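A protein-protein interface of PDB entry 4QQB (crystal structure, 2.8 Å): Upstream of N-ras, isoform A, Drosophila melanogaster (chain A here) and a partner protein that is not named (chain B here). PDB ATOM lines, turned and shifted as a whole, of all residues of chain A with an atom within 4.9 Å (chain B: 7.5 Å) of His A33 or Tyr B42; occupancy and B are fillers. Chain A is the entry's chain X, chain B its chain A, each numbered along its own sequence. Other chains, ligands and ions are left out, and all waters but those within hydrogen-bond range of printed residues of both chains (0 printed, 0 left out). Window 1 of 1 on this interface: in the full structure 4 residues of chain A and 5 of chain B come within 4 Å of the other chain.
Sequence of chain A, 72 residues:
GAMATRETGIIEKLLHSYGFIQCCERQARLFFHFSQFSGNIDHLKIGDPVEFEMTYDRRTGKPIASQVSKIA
The side-chain hydroxyl (OH) of Tyr B42 is in hydrogen-bond range of the backbone carbonyl oxygen (O) of Phe A34 (3.2 Å). The backbone carbonyl oxygen (O) of Tyr B42 is in hydrogen-bond range of the side-chain hydroxyl (OG) of Ser A35, 2.6 Å away.
Of the 9 printed residues of chain B, 1 touches a printed residue of chain A. Printed residues of chain B that touch a printed residue of chain A: Tyr B42. Among the printed residues, 3 pairs touch across the chains. Among the printed residues, no Asp or Glu carboxylate lies within 4 Å of a Lys or Arg side-chain nitrogen of the other chain.
OG of Ser A17 sits at hydrogen-bond distance from NE2 of His A33, at 3.0 Å. O of Ser A17 sits at hydrogen-bond distance from N of Phe A34 (3.0 Å). A ring nitrogen (ND1) of His A33 is in hydrogen-bond range of the side-chain hydroxyl of Ser A35 (2.7 Å).
O of Tyr B42 touches CE1 of His A33 (3.6 Å).
His A33 touches just one residue of chain B: Tyr B42. Printed residues of chain B within 4 Å of Phe A34: Tyr B42. Of the printed residues of chain B, Ser A35 touches Tyr B42 (2.6 Å). Arg B40 touches none of the printed residues of chain A. The nearest residue of chain B that does not touch His A33 is Asp B41 (5.8 Å). The nearest printed residue of chain A that does not touch Tyr B42 is Gln A36 (5.5 Å).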
ATOM      1  N   SER A  17     -32.093  -8.653  19.580  1.00  0.00           N
ATOM      2  CA  SER A  17     -31.737  -8.731  18.169  1.00  0.00           C
ATOM      3  C   SER A  17     -30.269  -9.061  17.874  1.00  0.00           C
ATOM      4  O   SER A  17     -29.935  -9.494  16.772  1.00  0.00           O
ATOM      5  CB  SER A  17     -32.074  -7.402  17.524  1.00  0.00           C
ATOM      6  OG  SER A  17     -32.108  -7.540  16.126  1.00  0.00           O
ATOM      7  N   TYR A  18     -29.390  -8.841  18.839  1.00  0.00           N
ATOM      8  CA  TYR A  18     -27.971  -9.067  18.633  1.00  0.00           C
ATOM      9  C   TYR A  18     -27.378  -9.589  19.918  1.00  0.00           C
ATOM     10  O   TYR A  18     -28.069  -9.697  20.929  1.00  0.00           O
ATOM     11  CB  TYR A  18     -27.279  -7.767  18.204  1.00  0.00           C
ATOM     12  CG  TYR A  18     -27.557  -6.569  19.095  1.00  0.00           C
ATOM     13  CD1 TYR A  18     -28.712  -5.811  18.935  1.00  0.00           C
ATOM     14  CD2 TYR A  18     -26.660  -6.187  20.087  1.00  0.00           C
ATOM     15  CE1 TYR A  18     -28.969  -4.716  19.740  1.00  0.00           C
ATOM     16  CE2 TYR A  18     -26.906  -5.090  20.895  1.00  0.00           C
ATOM     17  CZ  TYR A  18     -28.062  -4.360  20.717  1.00  0.00           C
ATOM     18  OH  TYR A  18     -28.316  -3.270  21.517  1.00  0.00           O
ATOM     19  N   PHE A  31     -19.338  -8.363  18.408  1.00  0.00           N
ATOM     20  CA  PHE A  31     -20.759  -8.147  18.173  1.00  0.00           C
ATOM     21  C   PHE A  31     -21.232  -9.147  17.118  1.00  0.00           C
ATOM     22  O   PHE A  31     -20.458  -9.565  16.261  1.00  0.00           O
ATOM     23  CB  PHE A  31     -20.963  -6.705  17.673  1.00  0.00           C
ATOM     24  CG  PHE A  31     -22.361  -6.402  17.204  1.00  0.00           C
ATOM     25  CD1 PHE A  31     -22.748  -6.685  15.900  1.00  0.00           C
ATOM     26  CD2 PHE A  31     -23.285  -5.817  18.060  1.00  0.00           C
ATOM     27  CE1 PHE A  31     -24.035  -6.408  15.468  1.00  0.00           C
ATOM     28  CE2 PHE A  31     -24.570  -5.538  17.632  1.00  0.00           C
ATOM     29  CZ  PHE A  31     -24.945  -5.833  16.334  1.00  0.00           C
ATOM     30  N   PHE A  32     -22.499  -9.530  17.183  1.00  0.00           N
ATOM     31  CA  PHE A  32     -23.108 -10.302  16.104  1.00  0.00           C
ATOM     32  C   PHE A  32     -24.610 -10.077  16.075  1.00  0.00           C
ATOM     33  O   PHE A  32     -25.248  -9.998  17.123  1.00  0.00           O
ATOM     34  CB  PHE A  32     -22.787 -11.797  16.240  1.00  0.00           C
ATOM     35  CG  PHE A  32     -23.666 -12.529  17.216  1.00  0.00           C
ATOM     36  CD1 PHE A  32     -23.316 -12.618  18.552  1.00  0.00           C
ATOM     37  CD2 PHE A  32     -24.843 -13.137  16.793  1.00  0.00           C
ATOM     38  CE1 PHE A  32     -24.121 -13.299  19.451  1.00  0.00           C
ATOM     39  CE2 PHE A  32     -25.659 -13.811  17.685  1.00  0.00           C
ATOM     40  CZ  PHE A  32     -25.295 -13.893  19.016  1.00  0.00           C
ATOM     41  N   HIS A  33     -25.164  -9.974  14.873  1.00  0.00           N
ATOM     42  CA  HIS A  33     -26.599  -9.786  14.693  1.00  0.00           C
ATOM     43  C   HIS A  33     -27.269 -11.140  14.441  1.00  0.00           C
ATOM     44  O   HIS A  33     -26.671 -12.032  13.838  1.00  0.00           O
ATOM     45  CB  HIS A  33     -26.857  -8.828  13.526  1.00  0.00           C
ATOM     46  CG  HIS A  33     -28.273  -8.352  13.439  1.00  0.00           C
ATOM     47  ND1 HIS A  33     -29.070  -8.582  12.340  1.00  0.00           N
ATOM     48  CD2 HIS A  33     -29.040  -7.670  14.321  1.00  0.00           C
ATOM     49  CE1 HIS A  33     -30.266  -8.060  12.546  1.00  0.00           C
ATOM     50  NE2 HIS A  33     -30.272  -7.494  13.738  1.00  0.00           N
ATOM     51  N   PHE A  34     -28.514 -11.290  14.885  1.00  0.00           N
ATOM     52  CA  PHE A  34     -29.224 -12.564  14.735  1.00  0.00           C
ATOM     53  C   PHE A  34     -29.454 -12.979  13.276  1.00  0.00           C
ATOM     54  O   PHE A  34     -29.779 -14.137  13.011  1.00  0.00           O
ATOM     55  CB  PHE A  34     -30.541 -12.560  15.527  1.00  0.00           C
ATOM     56  CG  PHE A  34     -30.355 -12.507  17.027  1.00  0.00           C
ATOM     57  CD1 PHE A  34     -29.098 -12.703  17.618  1.00  0.00           C
ATOM     58  CD2 PHE A  34     -31.448 -12.285  17.858  1.00  0.00           C
ATOM     59  CE1 PHE A  34     -28.945 -12.657  18.994  1.00  0.00           C
ATOM     60  CE2 PHE A  34     -31.296 -12.236  19.234  1.00  0.00           C
ATOM     61  CZ  PHE A  34     -30.045 -12.423  19.802  1.00  0.00           C
ATOM     62  N   SER A  35     -29.278 -12.045  12.345  1.00  0.00           N
ATOM     63  CA  SER A  35     -29.178 -12.370  10.926  1.00  0.00           C
ATOM     64  C   SER A  35     -28.097 -13.407  10.657  1.00  0.00           C
ATOM     65  O   SER A  35     -28.242 -14.232   9.761  1.00  0.00           O
ATOM     66  CB  SER A  35     -28.845 -11.124  10.113  1.00  0.00           C
ATOM     67  OG  SER A  35     -29.832 -10.132  10.284  1.00  0.00           O
ATOM     68  N   GLN A  36     -27.011 -13.352  11.417  1.00  0.00           N
ATOM     69  CA  GLN A  36     -25.903 -14.286  11.240  1.00  0.00           C
ATOM     70  C   GLN A  36     -26.059 -15.628  11.943  1.00  0.00           C
ATOM     71  O   GLN A  36     -25.224 -16.515  11.744  1.00  0.00           O
ATOM     72  CB  GLN A  36     -24.602 -13.634  11.706  1.00  0.00           C
ATOM     73  CG  GLN A  36     -24.237 -12.387  10.932  1.00  0.00           C
ATOM     74  CD  GLN A  36     -24.227 -12.633   9.443  1.00  0.00           C
ATOM     75  OE1 GLN A  36     -23.176 -12.873   8.851  1.00  0.00           O
ATOM     76  NE2 GLN A  36     -25.407 -12.600   8.831  1.00  0.00           N
ATOM     77  N   PHE A  37     -27.104 -15.784  12.756  1.00  0.00           N
ATOM     78  CA  PHE A  37     -27.320 -17.026  13.493  1.00  0.00           C
ATOM     79  C   PHE A  37     -28.208 -18.005  12.733  1.00  0.00           C
ATOM     80  O   PHE A  37     -29.107 -17.594  12.004  1.00  0.00           O
ATOM     81  CB  PHE A  37     -27.936 -16.741  14.853  1.00  0.00           C
ATOM     82  CG  PHE A  37     -27.916 -17.925  15.771  1.00  0.00           C
ATOM     83  CD1 PHE A  37     -26.723 -18.356  16.330  1.00  0.00           C
ATOM     84  CD2 PHE A  37     -29.083 -18.620  16.063  1.00  0.00           C
ATOM     85  CE1 PHE A  37     -26.693 -19.452  17.172  1.00  0.00           C
ATOM     86  CE2 PHE A  37     -29.060 -19.718  16.905  1.00  0.00           C
ATOM     87  CZ  PHE A  37     -27.862 -20.134  17.460  1.00  0.00           C
ATOM     88  N   MET B  39     -36.100   1.507  11.867  1.00  0.00           N
ATOM     89  CA  MET B  39     -36.345   0.442  10.906  1.00  0.00           C
ATOM     90  C   MET B  39     -35.169   0.254   9.989  1.00  0.00           C
ATOM     91  O   MET B  39     -34.648   1.221   9.439  1.00  0.00           O
ATOM     92  CB  MET B  39     -37.584   0.750  10.065  1.00  0.00           C
ATOM     93  CG  MET B  39     -38.782  -0.064  10.483  1.00  0.00           C
ATOM     94  SD  MET B  39     -38.964   0.050  12.256  1.00  0.00           S
ATOM     95  CE  MET B  39     -40.137  -1.259  12.511  1.00  0.00           C
ATOM     96  N   ARG B  40     -34.764  -0.996   9.806  1.00  0.00           N
ATOM     97  CA  ARG B  40     -33.661  -1.291   8.905  1.00  0.00           C
ATOM     98  C   ARG B  40     -33.819  -2.628   8.173  1.00  0.00           C
ATOM     99  O   ARG B  40     -34.679  -3.446   8.498  1.00  0.00           O
ATOM    100  CB  ARG B  40     -32.322  -1.199   9.651  1.00  0.00           C
ATOM    101  CG  ARG B  40     -32.416  -1.455  11.140  1.00  0.00           C
ATOM    102  CD  ARG B  40     -31.099  -1.159  11.838  1.00  0.00           C
ATOM    103  NE  ARG B  40     -30.993   0.239  12.247  1.00  0.00           N
ATOM    104  CZ  ARG B  40     -29.875   0.965  12.221  1.00  0.00           C
ATOM    105  NH1 ARG B  40     -28.731   0.452  11.784  1.00  0.00           N
ATOM    106  NH2 ARG B  40     -29.900   2.229  12.621  1.00  0.00           N
ATOM    107  N   ASP B  41     -32.998  -2.807   7.145  1.00  0.00           N
ATOM    108  CA  ASP B  41     -32.968  -4.040   6.385  1.00  0.00           C
ATOM    109  C   ASP B  41     -32.378  -5.128   7.270  1.00  0.00           C
ATOM    110  O   ASP B  41     -31.240  -5.021   7.714  1.00  0.00           O
ATOM    111  CB  ASP B  41     -32.103  -3.860   5.134  1.00  0.00           C
ATOM    112  CG  ASP B  41     -32.098  -5.084   4.248  1.00  0.00           C
ATOM    113  OD1 ASP B  41     -32.966  -5.172   3.362  1.00  0.00           O
ATOM    114  OD2 ASP B  41     -31.227  -5.955   4.434  1.00  0.00           O
ATOM    115  N   TYR B  42     -33.149  -6.173   7.530  1.00  0.00           N
ATOM    116  CA  TYR B  42     -32.699  -7.237   8.424  1.00  0.00           C
ATOM    117  C   TYR B  42     -31.311  -7.771   8.056  1.00  0.00           C
ATOM    118  O   TYR B  42     -30.473  -7.956   8.927  1.00  0.00           O
ATOM    119  CB  TYR B  42     -33.721  -8.380   8.444  1.00  0.00           C
ATOM    120  CG  TYR B  42     -33.368  -9.523   9.376  1.00  0.00           C
ATOM    121  CD1 TYR B  42     -33.479  -9.384  10.761  1.00  0.00           C
ATOM    122  CD2 TYR B  42     -32.932 -10.746   8.871  1.00  0.00           C
ATOM    123  CE1 TYR B  42     -33.158 -10.430  11.612  1.00  0.00           C
ATOM    124  CE2 TYR B  42     -32.613 -11.801   9.715  1.00  0.00           C
ATOM    125  CZ  TYR B  42     -32.725 -11.643  11.081  1.00  0.00           C
ATOM    126  OH  TYR B  42     -32.401 -12.694  11.910  1.00  0.00           O
ATOM    127  N   LYS B  43     -31.061  -7.987   6.769  1.00  0.00           N
ATOM    128  CA  LYS B  43     -29.862  -8.699   6.340  1.00  0.00           C
ATOM    129  C   LYS B  43     -28.616  -7.814   6.234  1.00  0.00           C
ATOM    130  O   LYS B  43     -27.521  -8.277   6.532  1.00  0.00           O
ATOM    131  CB  LYS B  43     -30.122  -9.428   5.020  1.00  0.00           C
ATOM    132  CG  LYS B  43     -31.263 -10.441   5.099  1.00  0.00           C
ATOM    133  CD  LYS B  43     -31.150 -11.553   4.059  1.00  0.00           C
ATOM    134  CE  LYS B  43     -31.020 -11.012   2.639  1.00  0.00           C
ATOM    135  NZ  LYS B  43     -32.062  -9.997   2.305  1.00  0.00           N
ATOM    136  N   THR B  44     -28.778  -6.562   5.807  1.00  0.00           N
ATOM    137  CA  THR B  44     -27.655  -5.608   5.719  1.00  0.00           C
ATOM    138  C   THR B  44     -27.660  -4.571   6.833  1.00  0.00           C
ATOM    139  O   THR B  44     -26.619  -4.014   7.175  1.00  0.00           O
ATOM    140  CB  THR B  44     -27.689  -4.826   4.403  1.00  0.00           C
ATOM    141  OG1 THR B  44     -28.885  -4.035   4.346  1.00  0.00           O
ATOM    142  CG2 THR B  44     -27.640  -5.780   3.224  1.00  0.00           C
ATOM    143  N   GLY B  45     -28.847  -4.282   7.360  1.00  0.00           N
ATOM    144  CA  GLY B  45     -28.998  -3.365   8.476  1.00  0.00           C
ATOM    145  C   GLY B  45     -29.080  -1.895   8.095  1.00  0.00           C
ATOM    146  O   GLY B  45     -29.154  -1.046   8.976  1.00  0.00           O
ATOM    147  N   TYR B  46     -29.043  -1.571   6.807  1.00  0.00           N
ATOM    148  CA  TYR B  46     -29.179  -0.176   6.382  1.00  0.00           C
ATOM    149  C   TYR B  46     -30.533   0.384   6.836  1.00  0.00           C
ATOM    150  O   TYR B  46     -31.535  -0.341   6.850  1.00  0.00           O
ATOM    151  CB  TYR B  46     -29.031  -0.055   4.862  1.00  0.00           C
ATOM    152  CG  TYR B  46     -27.597  -0.080   4.375  1.00  0.00           C
ATOM    153  CD1 TYR B  46     -26.797   1.058   4.457  1.00  0.00           C
ATOM    154  CD2 TYR B  46     -27.040  -1.232   3.821  1.00  0.00           C
ATOM    155  CE1 TYR B  46     -25.486   1.052   4.008  1.00  0.00           C
ATOM    156  CE2 TYR B  46     -25.724  -1.246   3.372  1.00  0.00           C
ATOM    157  CZ  TYR B  46     -24.957  -0.097   3.462  1.00  0.00           C
ATOM    158  OH  TYR B  46     -23.651  -0.087   3.033  1.00  0.00           O
ATOM    159  N   PHE B  48     -34.034   2.237   6.998  1.00  0.00           N
ATOM    160  CA  PHE B  48     -35.131   2.626   6.114  1.00  0.00           C
ATOM    161  C   PHE B  48     -35.476   4.099   6.260  1.00  0.00           C
ATOM    162  O   PHE B  48     -36.331   4.600   5.543  1.00  0.00           O
ATOM    163  CB  PHE B  48     -36.386   1.785   6.365  1.00  0.00           C
ATOM    164  CG  PHE B  48     -36.307   0.387   5.808  1.00  0.00           C
ATOM    165  CD1 PHE B  48     -35.992   0.173   4.473  1.00  0.00           C
ATOM    166  CD2 PHE B  48     -36.573  -0.714   6.611  1.00  0.00           C
ATOM    167  CE1 PHE B  48     -35.921  -1.107   3.959  1.00  0.00           C
ATOM    168  CE2 PHE B  48     -36.504  -1.997   6.103  1.00  0.00           C
ATOM    169  CZ  PHE B  48     -36.179  -2.194   4.774  1.00  0.00           C
